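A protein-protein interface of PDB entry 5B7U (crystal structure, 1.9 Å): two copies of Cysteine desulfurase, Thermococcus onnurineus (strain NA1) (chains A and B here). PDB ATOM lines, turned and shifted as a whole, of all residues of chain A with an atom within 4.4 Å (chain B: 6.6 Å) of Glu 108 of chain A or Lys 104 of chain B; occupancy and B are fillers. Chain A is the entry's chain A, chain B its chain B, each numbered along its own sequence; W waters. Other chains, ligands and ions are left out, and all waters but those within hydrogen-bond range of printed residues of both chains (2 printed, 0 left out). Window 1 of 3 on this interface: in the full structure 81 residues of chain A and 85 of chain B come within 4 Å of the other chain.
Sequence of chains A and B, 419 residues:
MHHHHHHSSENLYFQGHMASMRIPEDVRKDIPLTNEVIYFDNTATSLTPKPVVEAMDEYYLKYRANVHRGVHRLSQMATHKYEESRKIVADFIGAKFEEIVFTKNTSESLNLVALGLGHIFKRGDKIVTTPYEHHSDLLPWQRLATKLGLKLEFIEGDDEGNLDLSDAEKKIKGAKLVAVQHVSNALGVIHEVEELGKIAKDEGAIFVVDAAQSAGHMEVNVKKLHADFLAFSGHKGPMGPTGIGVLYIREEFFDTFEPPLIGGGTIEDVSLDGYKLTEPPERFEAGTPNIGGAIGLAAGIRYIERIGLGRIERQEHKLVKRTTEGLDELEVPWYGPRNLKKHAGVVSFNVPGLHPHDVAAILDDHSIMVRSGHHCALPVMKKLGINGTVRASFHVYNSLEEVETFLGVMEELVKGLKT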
ATOM      1  N   THR A 103     -22.633   7.089 -14.582  1.00  0.00           N
ATOM      2  CA  THR A 103     -22.552   8.464 -14.888  1.00  0.00           C
ATOM      3  C   THR A 103     -21.794   9.117 -13.720  1.00  0.00           C
ATOM      4  O   THR A 103     -21.349   8.414 -12.786  1.00  0.00           O
ATOM      5  CB  THR A 103     -23.974   9.048 -14.949  1.00  0.00           C
ATOM      6  OG1 THR A 103     -24.546   8.888 -13.655  1.00  0.00           O
ATOM      7  CG2 THR A 103     -24.811   8.265 -16.012  1.00  0.00           C
ATOM      8  N   LYS A 104     -21.675  10.425 -13.733  1.00  0.00           N
ATOM      9  CA  LYS A 104     -21.018  11.135 -12.630  1.00  0.00           C
ATOM     10  C   LYS A 104     -21.946  11.376 -11.441  1.00  0.00           C
ATOM     11  O   LYS A 104     -21.484  11.499 -10.310  1.00  0.00           O
ATOM     12  CB  LYS A 104     -20.351  12.431 -13.101  1.00  0.00           C
ATOM     13  CG  LYS A 104     -21.141  13.652 -13.006  1.00  0.00           C
ATOM     14  CD  LYS A 104     -20.289  14.947 -13.175  1.00  0.00           C
ATOM     15  CE  LYS A 104     -19.837  15.057 -14.608  1.00  0.00           C
ATOM     16  NZ  LYS A 104     -20.974  15.073 -15.612  1.00  0.00           N
ATOM     17  N   ASN A 105     -23.252  11.426 -11.691  1.00  0.00           N
ATOM     18  CA  ASN A 105     -24.191  11.726 -10.611  1.00  0.00           C
ATOM     19  C   ASN A 105     -25.617  11.610 -11.175  1.00  0.00           C
ATOM     20  O   ASN A 105     -25.830  11.474 -12.426  1.00  0.00           O
ATOM     21  CB  ASN A 105     -23.950  13.138 -10.001  1.00  0.00           C
ATOM     22  CG  ASN A 105     -23.979  14.277 -11.013  1.00  0.00           C
ATOM     23  OD1 ASN A 105     -24.636  14.255 -12.075  1.00  0.00           O
ATOM     24  ND2 ASN A 105     -23.255  15.318 -10.672  1.00  0.00           N
ATOM     25  N   THR A 106     -26.579  11.757 -10.294  1.00  0.00           N
ATOM     26  CA  THR A 106     -27.991  11.789 -10.703  1.00  0.00           C
ATOM     27  C   THR A 106     -28.291  12.835 -11.744  1.00  0.00           C
ATOM     28  O   THR A 106     -29.009  12.543 -12.700  1.00  0.00           O
ATOM     29  CB  THR A 106     -28.929  11.980  -9.519  1.00  0.00           C
ATOM     30  OG1 THR A 106     -28.833  10.871  -8.674  1.00  0.00           O
ATOM     31  CG2 THR A 106     -30.352  12.104  -9.938  1.00  0.00           C
ATOM     32  N   SER A 107     -27.715  14.017 -11.583  1.00  0.00           N
ATOM     33  CA  SER A 107     -27.925  15.121 -12.532  1.00  0.00           C
ATOM     34  C   SER A 107     -27.507  14.806 -13.971  1.00  0.00           C
ATOM     35  O   SER A 107     -28.316  15.017 -14.896  1.00  0.00           O
ATOM     36  CB  SER A 107     -27.232  16.376 -12.037  1.00  0.00           C
ATOM     37  OG  SER A 107     -27.731  16.710 -10.706  1.00  0.00           O
ATOM     38  N   GLU A 108     -26.357  14.151 -14.137  1.00  0.00           N
ATOM     39  CA  GLU A 108     -25.950  13.708 -15.452  1.00  0.00           C
ATOM     40  C   GLU A 108     -26.940  12.676 -15.961  1.00  0.00           C
ATOM     41  O   GLU A 108     -27.410  12.786 -17.089  1.00  0.00           O
ATOM     42  CB  GLU A 108     -24.577  13.109 -15.427  1.00  0.00           C
ATOM     43  CG  GLU A 108     -24.127  12.675 -16.822  1.00  0.00           C
ATOM     44  CD  GLU A 108     -22.758  11.961 -16.785  1.00  0.00           C
ATOM     45  OE1 GLU A 108     -21.951  12.276 -15.912  1.00  0.00           O
ATOM     46  OE2 GLU A 108     -22.465  11.073 -17.645  1.00  0.00           O
ATOM     47  N   SER A 109     -27.253  11.692 -15.124  1.00  0.00           N
ATOM     48  CA  SER A 109     -28.220  10.619 -15.498  1.00  0.00           C
ATOM     49  C   SER A 109     -29.542  11.205 -16.027  1.00  0.00           C
ATOM     50  O   SER A 109     -30.018  10.842 -17.144  1.00  0.00           O
ATOM     51  CB  SER A 109     -28.513   9.679 -14.319  1.00  0.00           C
ATOM     52  OG  SER A 109     -27.378   8.986 -13.890  1.00  0.00           O
ATOM     53  N   LEU A 110     -30.113  12.145 -15.298  1.00  0.00           N
ATOM     54  CA  LEU A 110     -31.394  12.748 -15.748  1.00  0.00           C
ATOM     55  C   LEU A 110     -31.303  13.556 -17.059  1.00  0.00           C
ATOM     56  O   LEU A 110     -32.158  13.449 -17.961  1.00  0.00           O
ATOM     57  CB  LEU A 110     -32.024  13.570 -14.624  1.00  0.00           C
ATOM     58  CG  LEU A 110     -32.531  12.754 -13.449  1.00  0.00           C
ATOM     59  CD1 LEU A 110     -32.903  13.731 -12.350  1.00  0.00           C
ATOM     60  CD2 LEU A 110     -33.736  11.884 -13.750  1.00  0.00           C
ATOM     61  N   ASN A 111     -30.233  14.309 -17.195  1.00  0.00           N
ATOM     62  CA  ASN A 111     -29.952  15.067 -18.402  1.00  0.00           C
ATOM     63  C   ASN A 111     -29.762  14.077 -19.546  1.00  0.00           C
ATOM     64  O   ASN A 111     -30.297  14.275 -20.582  1.00  0.00           O
ATOM     65  CB  ASN A 111     -28.731  15.950 -18.249  1.00  0.00           C
ATOM     66  CG  ASN A 111     -29.070  17.305 -17.672  1.00  0.00           C
ATOM     67  OD1 ASN A 111     -29.386  18.219 -18.370  1.00  0.00           O
ATOM     68  ND2 ASN A 111     -29.059  17.384 -16.388  1.00  0.00           N
ATOM     69  N   LEU A 112     -29.004  13.004 -19.323  1.00  0.00           N
ATOM     70  CA  LEU A 112     -28.863  11.990 -20.390  1.00  0.00           C
ATOM     71  C   LEU A 112     -30.231  11.418 -20.877  1.00  0.00           C
ATOM     72  O   LEU A 112     -30.420  11.199 -22.118  1.00  0.00           O
ATOM     73  CB  LEU A 112     -27.977  10.846 -19.978  1.00  0.00           C
ATOM     74  CG  LEU A 112     -26.529  11.234 -19.711  1.00  0.00           C
ATOM     75  CD1 LEU A 112     -25.799   9.996 -19.199  1.00  0.00           C
ATOM     76  CD2 LEU A 112     -25.899  11.781 -20.938  1.00  0.00           C
ATOM     77  N   LEU A 261     -23.509  10.683 -25.240  1.00  0.00           N
ATOM     78  CA  LEU A 261     -22.078  10.779 -25.199  1.00  0.00           C
ATOM     79  C   LEU A 261     -21.526   9.533 -25.874  1.00  0.00           C
ATOM     80  O   LEU A 261     -21.882   8.387 -25.501  1.00  0.00           O
ATOM     81  CB  LEU A 261     -21.596  10.790 -23.759  1.00  0.00           C
ATOM     82  CG  LEU A 261     -22.235  11.833 -22.852  1.00  0.00           C
ATOM     83  CD1 LEU A 261     -21.760  11.681 -21.414  1.00  0.00           C
ATOM     84  CD2 LEU A 261     -22.000  13.215 -23.319  1.00  0.00           C
ATOM     85  N   PHE B 102     -15.163  20.812 -14.565  1.00  0.00           N
ATOM     86  CA  PHE B 102     -14.875  19.354 -14.265  1.00  0.00           C
ATOM     87  C   PHE B 102     -15.949  18.479 -14.905  1.00  0.00           C
ATOM     88  O   PHE B 102     -17.180  18.771 -14.862  1.00  0.00           O
ATOM     89  CB  PHE B 102     -14.754  19.096 -12.762  1.00  0.00           C
ATOM     90  CG  PHE B 102     -13.551  19.689 -12.151  1.00  0.00           C
ATOM     91  CD1 PHE B 102     -12.311  19.266 -12.554  1.00  0.00           C
ATOM     92  CD2 PHE B 102     -13.624  20.645 -11.122  1.00  0.00           C
ATOM     93  CE1 PHE B 102     -11.155  19.806 -11.992  1.00  0.00           C
ATOM     94  CE2 PHE B 102     -12.488  21.149 -10.534  1.00  0.00           C
ATOM     95  CZ  PHE B 102     -11.244  20.756 -10.988  1.00  0.00           C
ATOM     96  N   THR B 103     -15.433  17.388 -15.489  1.00  0.00           N
ATOM     97  CA  THR B 103     -16.204  16.382 -16.240  1.00  0.00           C
ATOM     98  C   THR B 103     -15.710  15.002 -15.719  1.00  0.00           C
ATOM     99  O   THR B 103     -14.849  14.938 -14.829  1.00  0.00           O
ATOM    100  CB  THR B 103     -15.891  16.491 -17.771  1.00  0.00           C
ATOM    101  OG1 THR B 103     -14.505  16.176 -17.997  1.00  0.00           O
ATOM    102  CG2 THR B 103     -16.166  17.931 -18.224  1.00  0.00           C
ATOM    103  N   LYS B 104     -16.254  13.913 -16.255  1.00  0.00           N
ATOM    104  CA  LYS B 104     -15.783  12.572 -15.840  1.00  0.00           C
ATOM    105  C   LYS B 104     -14.506  12.146 -16.529  1.00  0.00           C
ATOM    106  O   LYS B 104     -13.786  11.349 -15.991  1.00  0.00           O
ATOM    107  CB  LYS B 104     -16.899  11.488 -15.971  1.00  0.00           C
ATOM    108  CG  LYS B 104     -16.893  10.742 -17.250  1.00  0.00           C
ATOM    109  CD  LYS B 104     -17.893   9.511 -17.298  1.00  0.00           C
ATOM    110  CE  LYS B 104     -19.338   9.926 -17.134  1.00  0.00           C
ATOM    111  NZ  LYS B 104     -19.717  11.025 -18.112  1.00  0.00           N
ATOM    112  N   ASN B 105     -14.259  12.636 -17.740  1.00  0.00           N
ATOM    113  CA  ASN B 105     -13.095  12.255 -18.534  1.00  0.00           C
ATOM    114  C   ASN B 105     -13.024  13.166 -19.798  1.00  0.00           C
ATOM    115  O   ASN B 105     -13.927  13.972 -20.088  1.00  0.00           O
ATOM    116  CB  ASN B 105     -13.157  10.781 -18.891  1.00  0.00           C
ATOM    117  CG  ASN B 105     -14.445  10.383 -19.616  1.00  0.00           C
ATOM    118  OD1 ASN B 105     -15.089  11.172 -20.312  1.00  0.00           O
ATOM    119  ND2 ASN B 105     -14.813   9.126 -19.481  1.00  0.00           N
ATOM    120  N   THR B 106     -11.938  13.010 -20.527  1.00  0.00           N
ATOM    121  CA  THR B 106     -11.780  13.675 -21.798  1.00  0.00           C
ATOM    122  C   THR B 106     -12.922  13.413 -22.745  1.00  0.00           C
ATOM    123  O   THR B 106     -13.388  14.329 -23.425  1.00  0.00           O
ATOM    124  CB  THR B 106     -10.510  13.230 -22.465  1.00  0.00           C
ATOM    125  OG1 THR B 106      -9.435  13.715 -21.679  1.00  0.00           O
ATOM    126  CG2 THR B 106     -10.385  13.733 -23.858  1.00  0.00           C
ATOM    127  N   SER B 107     -13.380  12.159 -22.814  1.00  0.00           N
ATOM    128  CA  SER B 107     -14.481  11.878 -23.751  1.00  0.00           C
ATOM    129  C   SER B 107     -15.710  12.704 -23.485  1.00  0.00           C
ATOM    130  O   SER B 107     -16.340  13.230 -24.415  1.00  0.00           O
ATOM    131  CB  SER B 107     -14.743  10.359 -23.810  1.00  0.00           C
ATOM    132  OG  SER B 107     -13.535   9.609 -23.997  1.00  0.00           O
ATOM    133  N   GLU B 108     -16.114  12.821 -22.203  1.00  0.00           N
ATOM    134  CA  GLU B 108     -17.252  13.652 -21.862  1.00  0.00           C
ATOM    135  C   GLU B 108     -16.973  15.128 -22.305  1.00  0.00           C
ATOM    136  O   GLU B 108     -17.840  15.772 -22.898  1.00  0.00           O
ATOM    137  CB  GLU B 108     -17.540  13.626 -20.352  1.00  0.00           C
ATOM    138  CG  GLU B 108     -18.712  14.583 -19.956  1.00  0.00           C
ATOM    139  CD  GLU B 108     -19.050  14.605 -18.450  1.00  0.00           C
ATOM    140  OE1 GLU B 108     -18.642  13.641 -17.700  1.00  0.00           O
ATOM    141  OE2 GLU B 108     -19.689  15.621 -18.027  1.00  0.00           O
ATOM    142  N   SER B 109     -15.797  15.608 -21.981  1.00  0.00           N
ATOM    143  CA  SER B 109     -15.363  16.941 -22.323  1.00  0.00           C
ATOM    144  C   SER B 109     -15.592  17.185 -23.811  1.00  0.00           C
ATOM    145  O   SER B 109     -16.261  18.092 -24.175  1.00  0.00           O
ATOM    146  CB  SER B 109     -13.906  17.106 -21.910  1.00  0.00           C
ATOM    147  OG  SER B 109     -13.789  17.206 -20.531  1.00  0.00           O
ATOM    148  N   SER B 233      -7.743  14.266 -19.167  1.00  0.00           N
ATOM    149  CA  SER B 233      -8.167  13.306 -18.181  1.00  0.00           C
ATOM    150  C   SER B 233      -7.231  13.178 -16.989  1.00  0.00           C
ATOM    151  O   SER B 233      -6.082  12.957 -17.145  1.00  0.00           O
ATOM    152  CB  SER B 233      -8.252  11.930 -18.814  1.00  0.00           C
ATOM    153  OG  SER B 233      -9.204  11.872 -19.817  1.00  0.00           O
ATOM    154  N   GLY B 234      -7.789  13.245 -15.794  1.00  0.00           N
ATOM    155  CA  GLY B 234      -6.993  13.133 -14.619  1.00  0.00           C
ATOM    156  C   GLY B 234      -6.236  11.833 -14.405  1.00  0.00           C
ATOM    157  O   GLY B 234      -5.217  11.829 -13.822  1.00  0.00           O
ATOM    158  N   HIS B 235      -6.798  10.732 -14.860  1.00  0.00           N
ATOM    159  CA  HIS B 235      -6.232   9.426 -14.647  1.00  0.00           C
ATOM    160  C   HIS B 235      -5.040   9.031 -15.510  1.00  0.00           C
ATOM    161  O   HIS B 235      -4.478   7.994 -15.325  1.00  0.00           O
ATOM    162  CB  HIS B 235      -7.309   8.359 -14.778  1.00  0.00           C
ATOM    163  CG  HIS B 235      -7.833   8.219 -16.162  1.00  0.00           C
ATOM    164  ND1 HIS B 235      -7.353   7.300 -17.034  1.00  0.00           N
ATOM    165  CD2 HIS B 235      -8.819   8.866 -16.805  1.00  0.00           C
ATOM    166  CE1 HIS B 235      -8.009   7.391 -18.168  1.00  0.00           C
ATOM    167  NE2 HIS B 235      -8.896   8.343 -18.060  1.00  0.00           N
ATOM    168  N1  LLP B 236      -7.855  11.230 -26.575  1.00  0.00           N
ATOM    169  C2  LLP B 236      -6.642  10.742 -26.480  1.00  0.00           C
ATOM    170  C2' LLP B 236      -5.574  11.242 -27.407  1.00  0.00           C
ATOM    171  C3  LLP B 236      -6.353   9.722 -25.474  1.00  0.00           C
ATOM    172  O3  LLP B 236      -5.187   9.168 -25.303  1.00  0.00           O
ATOM    173  C4  LLP B 236      -7.463   9.305 -24.614  1.00  0.00           C
ATOM    174  C4' LLP B 236      -7.247   8.248 -23.592  1.00  0.00           C
ATOM    175  C5  LLP B 236      -8.769   9.911 -24.839  1.00  0.00           C
ATOM    176  C6  LLP B 236      -8.878  10.856 -25.830  1.00  0.00           C
ATOM    177  C5' LLP B 236      -9.969   9.520 -23.992  1.00  0.00           C
ATOM    178  OP4 LLP B 236      -9.757   9.647 -22.617  1.00  0.00           O
ATOM    179  P   LLP B 236     -10.798   9.103 -21.560  1.00  0.00           P
ATOM    180  OP1 LLP B 236     -12.049   9.690 -21.830  1.00  0.00           O
ATOM    181  OP2 LLP B 236     -10.273   9.530 -20.353  1.00  0.00           O
ATOM    182  OP3 LLP B 236     -10.784   7.677 -21.737  1.00  0.00           O
ATOM    183  N   LLP B 236      -4.706   9.879 -16.461  1.00  0.00           N
ATOM    184  CA  LLP B 236      -3.580   9.615 -17.326  1.00  0.00           C
ATOM    185  CB  LLP B 236      -3.883   9.917 -18.779  1.00  0.00           C
ATOM    186  CG  LLP B 236      -4.871   8.921 -19.348  1.00  0.00           C
ATOM    187  CD  LLP B 236      -5.353   9.373 -20.694  1.00  0.00           C
ATOM    188  CE  LLP B 236      -6.204   8.313 -21.364  1.00  0.00           C
ATOM    189  NZ  LLP B 236      -6.132   8.467 -22.776  1.00  0.00           N
ATOM    190  C   LLP B 236      -2.326  10.305 -16.772  1.00  0.00           C
ATOM    191  O   LLP B 236      -2.024  10.131 -15.645  1.00  0.00           O
ATOM    192  N   PRO B 241      -6.926  10.453 -10.005  1.00  0.00           N
ATOM    193  CA  PRO B 241      -7.844   9.298  -9.950  1.00  0.00           C
ATOM    194  C   PRO B 241      -8.681   9.204 -11.237  1.00  0.00           C
ATOM    195  O   PRO B 241      -8.706  10.117 -12.047  1.00  0.00           O
ATOM    196  CB  PRO B 241      -8.715   9.618  -8.747  1.00  0.00           C
ATOM    197  CG  PRO B 241      -8.805  11.093  -8.755  1.00  0.00           C
ATOM    198  CD  PRO B 241      -7.402  11.580  -9.199  1.00  0.00           C
ATOM    199  N   THR B 242      -9.423   8.101 -11.382  1.00  0.00           N
ATOM    200  CA  THR B 242     -10.413   7.970 -12.422  1.00  0.00           C
ATOM    201  C   THR B 242     -11.604   8.845 -12.085  1.00  0.00           C
ATOM    202  O   THR B 242     -11.761   9.279 -10.941  1.00  0.00           O
ATOM    203  CB  THR B 242     -10.921   6.493 -12.551  1.00  0.00           C
ATOM    204  OG1 THR B 242     -11.510   6.079 -11.312  1.00  0.00           O
ATOM    205  CG2 THR B 242      -9.726   5.594 -12.850  1.00  0.00           C
ATOM    206  N   GLY B 243     -12.456   9.020 -13.080  1.00  0.00           N
ATOM    207  CA  GLY B 243     -13.708   9.745 -12.933  1.00  0.00           C
ATOM    208  C   GLY B 243     -13.553  11.271 -12.854  1.00  0.00           C
ATOM    209  O   GLY B 243     -14.481  11.954 -12.478  1.00  0.00           O
ATOM    210  N   ILE B 244     -12.379  11.803 -13.221  1.00  0.00           N
ATOM    211  CA  ILE B 244     -12.253  13.266 -13.236  1.00  0.00           C
ATOM    212  C   ILE B 244     -11.547  13.667 -14.518  1.00  0.00           C
ATOM    213  O   ILE B 244     -10.409  13.228 -14.767  1.00  0.00           O
ATOM    214  CB  ILE B 244     -11.566  13.760 -11.966  1.00  0.00           C
ATOM    215  CG1 ILE B 244     -11.600  15.316 -11.797  1.00  0.00           C
ATOM    216  CG2 ILE B 244     -10.122  13.333 -11.864  1.00  0.00           C
ATOM    217  CD1 ILE B 244     -12.992  15.843 -11.545  1.00  0.00           C
ATOM    218  N   GLY B 245     -12.204  14.532 -15.234  1.00  0.00           N
ATOM    219  CA  GLY B 245     -11.742  15.126 -16.450  1.00  0.00           C
ATOM    220  C   GLY B 245     -11.873  16.628 -16.374  1.00  0.00           C
ATOM    221  O   GLY B 245     -12.493  17.151 -15.508  1.00  0.00           O
ATOM    222  N   VAL B 246     -11.265  17.290 -17.337  1.00  0.00           N
ATOM    223  CA  VAL B 246     -11.304  18.729 -17.405  1.00  0.00           C
ATOM    224  C   VAL B 246     -11.729  19.196 -18.802  1.00  0.00           C
ATOM    225  O   VAL B 246     -11.373  18.583 -19.778  1.00  0.00           O
ATOM    226  CB  VAL B 246      -9.934  19.307 -17.056  1.00  0.00           C
ATOM    227  CG1 VAL B 246      -9.829  20.789 -17.400  1.00  0.00           C
ATOM    228  CG2 VAL B 246      -9.590  19.028 -15.621  1.00  0.00           C
ATOM    229  N   LEU B 261     -25.509  19.933 -19.932  1.00  0.00           N
ATOM    230  CA  LEU B 261     -26.120  19.394 -18.701  1.00  0.00           C
ATOM    231  C   LEU B 261     -26.453  20.490 -17.740  1.00  0.00           C
ATOM    232  O   LEU B 261     -25.553  21.254 -17.354  1.00  0.00           O
ATOM    233  CB  LEU B 261     -25.142  18.442 -18.013  1.00  0.00           C
ATOM    234  CG  LEU B 261     -24.369  17.517 -18.943  1.00  0.00           C
ATOM    235  CD1 LEU B 261     -23.319  16.755 -18.111  1.00  0.00           C
ATOM    236  CD2 LEU B 261     -25.305  16.573 -19.652  1.00  0.00           C
ATOM    237  N   ALA B 286     -23.290  20.384 -13.649  1.00  0.00           N
ATOM    238  CA  ALA B 286     -24.622  20.018 -13.121  1.00  0.00           C
ATOM    239  C   ALA B 286     -24.485  18.899 -12.108  1.00  0.00           C
ATOM    240  O   ALA B 286     -23.803  17.880 -12.364  1.00  0.00           O
ATOM    241  CB  ALA B 286     -25.545  19.554 -14.198  1.00  0.00           C
ATOM    242  N   GLY B 287     -25.089  19.150 -10.968  1.00  0.00           N
ATOM    243  CA  GLY B 287     -25.142  18.235  -9.835  1.00  0.00           C
ATOM    244  C   GLY B 287     -23.862  18.246  -9.018  1.00  0.00           C
ATOM    245  O   GLY B 287     -22.880  18.975  -9.335  1.00  0.00           O
ATOM    246  N   ASN B 290     -17.446  15.679  -8.727  1.00  0.00           N
ATOM    247  CA  ASN B 290     -16.631  14.624  -8.181  1.00  0.00           C
ATOM    248  C   ASN B 290     -15.608  15.317  -7.252  1.00  0.00           C
ATOM    249  O   ASN B 290     -14.475  15.487  -7.586  1.00  0.00           O
ATOM    250  CB  ASN B 290     -15.983  13.769  -9.250  1.00  0.00           C
ATOM    251  CG  ASN B 290     -15.228  12.620  -8.668  1.00  0.00           C
ATOM    252  OD1 ASN B 290     -15.200  12.448  -7.480  1.00  0.00           O
ATOM    253  ND2 ASN B 290     -14.619  11.819  -9.527  1.00  0.00           N
HETATM  254  O   HOH W   1     -23.284  16.372 -14.483  1.00  0.00           O
HETATM  255  O   HOH W   2     -19.585  18.012 -16.162  1.00  0.00           O
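NZ of Lys 104 of chain A lies within salt-bridge range of OE2 of Glu 108 of chain B (2.8 Å).
The side-chain amide nitrogen (ND2) of Asn 105 of chain A sits at hydrogen-bond distance from the backbone carbonyl oxygen (O) of Ala 286 of chain B, at 3.1 Å.
OE2 of Glu 108 of chain A lies within salt-bridge range of NZ of Lys 104 of chain B.
The backbone carbonyl oxygen (O) of Asn 105 of chain A is in hydrogen-bond range of the side-chain hydroxyl (OG1) of Thr 103 of chain A (3.1 Å).
OE1 of Glu 108 of chain A lies within salt-bridge range of NZ of Lys 104 of chain A (3.0 Å).
The side-chain amide oxygen (OD1) of Asn 105 of chain A lies within hydrogen-bond range of the backbone NH (N) of Ser 107 of chain A, 3.1 Å away.
The backbone carbonyl oxygen (O) of Asn 105 of chain A is in hydrogen-bond range of the side-chain hydroxyl (OG) of Ser 109 of chain A.
The side-chain amino group of Lys 104 of chain B is in salt-bridge range of the side-chain carboxylate of Glu 108 of chain B, 2.9 Å away.
N of Ile 244 of chain B is in hydrogen-bond range of O of Lys 104 of chain B, at 3.1 Å.
CD1 of Leu 261 of chain B touches NZ of Lys 104 of chain A (3.8 Å).
C of Gly 287 of chain B touches ND2 of Asn 105 of chain A (3.4 Å).
Ala 286 of chain B touches Ser 107 of chain A.
CA of Gly 287 of chain B touches OG of Ser 107 of chain A, 3.1 Å away.
Leu 261 of chain B touches Asn 111 of chain A (CA to OD1, 3.5 Å).
Lys 104 of chain B touches Leu 261 of chain A (NZ to CD1, 3.9 Å).
Of the printed residues of chain B, Glu 108 of chain A touches Lys 104.
Of the printed residues of chain A, Glu 108 of chain B touches Lys 104.
Printed residues of chain B within 4 Å of Asn 111 of chain A: Leu 261 (3.5 Å).
Printed residues of chain A within 4 Å of Leu 261 of chain B: Lys 104 (3.8 Å) and Asn 111 (3.5 Å).
Of the printed residues of chain B, Leu 261 of chain A touches Lys 104.
Thr 106 of chain A touches none of the printed residues of chain B.
The nearest residue of chain A that does not touch Lys 104 of chain B is Lys 104 of chain A (4.1 Å).
The nearest printed residue of chain B that does not touch Asn 111 of chain A is Ala 286 of chain B (4.7 Å).
Of the 22 printed residues of chain B, 5 touch a printed residue of chain A.
Hydrophobic or aromatic side chains of chain B within 4 Å of the printed part of chain A: Leu 261.
Printed residues of chain A that touch a printed residue of chain B: Lys 104, Asn 105, Ser 107, Glu 108, Asn 111 and Leu 261.
Among the printed residues, 9 pairs touch across the chains.
Among the printed residues, Asp or Glu carboxylates within 4 Å of a Lys or Arg side-chain nitrogen of the other chain: Lys 104 of chain A with Glu 108 of chain B (2.8 Å) and Glu 108 of chain A with Lys 104 of chain B (2.8 Å).
Lys 104 of chain A touches Glu 108 of chain B, and with the chains exchanged Glu 108 of chain A touches Lys 104 of chain B.
Lys 104 of chain A touches Leu 261 of chain B, and with the chains exchanged Leu 261 of chain A touches Lys 104 of chain B.
8 positions are printed for both chains.
Of the 9 pairs that touch across the chains among the printed residues, 4 have their exchanged pair printed and touching as well.
Water W1 lies within hydrogen-bond range of the backbone carbonyl oxygen of Ala 286 of chain B (2.7 Å), the side-chain amino group of Lys 104 of chain A (2.9 Å) and the side-chain amide oxygen of Asn 105 of chain A (3.5 Å).
Water W2 lies within hydrogen-bond range of the backbone carbonyl oxygen (O) of Phe 102 of chain B (2.8 Å), the side-chain carboxylate (OE2) of Glu 108 of chain B (3.0 Å) and the side-chain amino group (NZ) of Lys 104 of chain A (3.3 Å).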
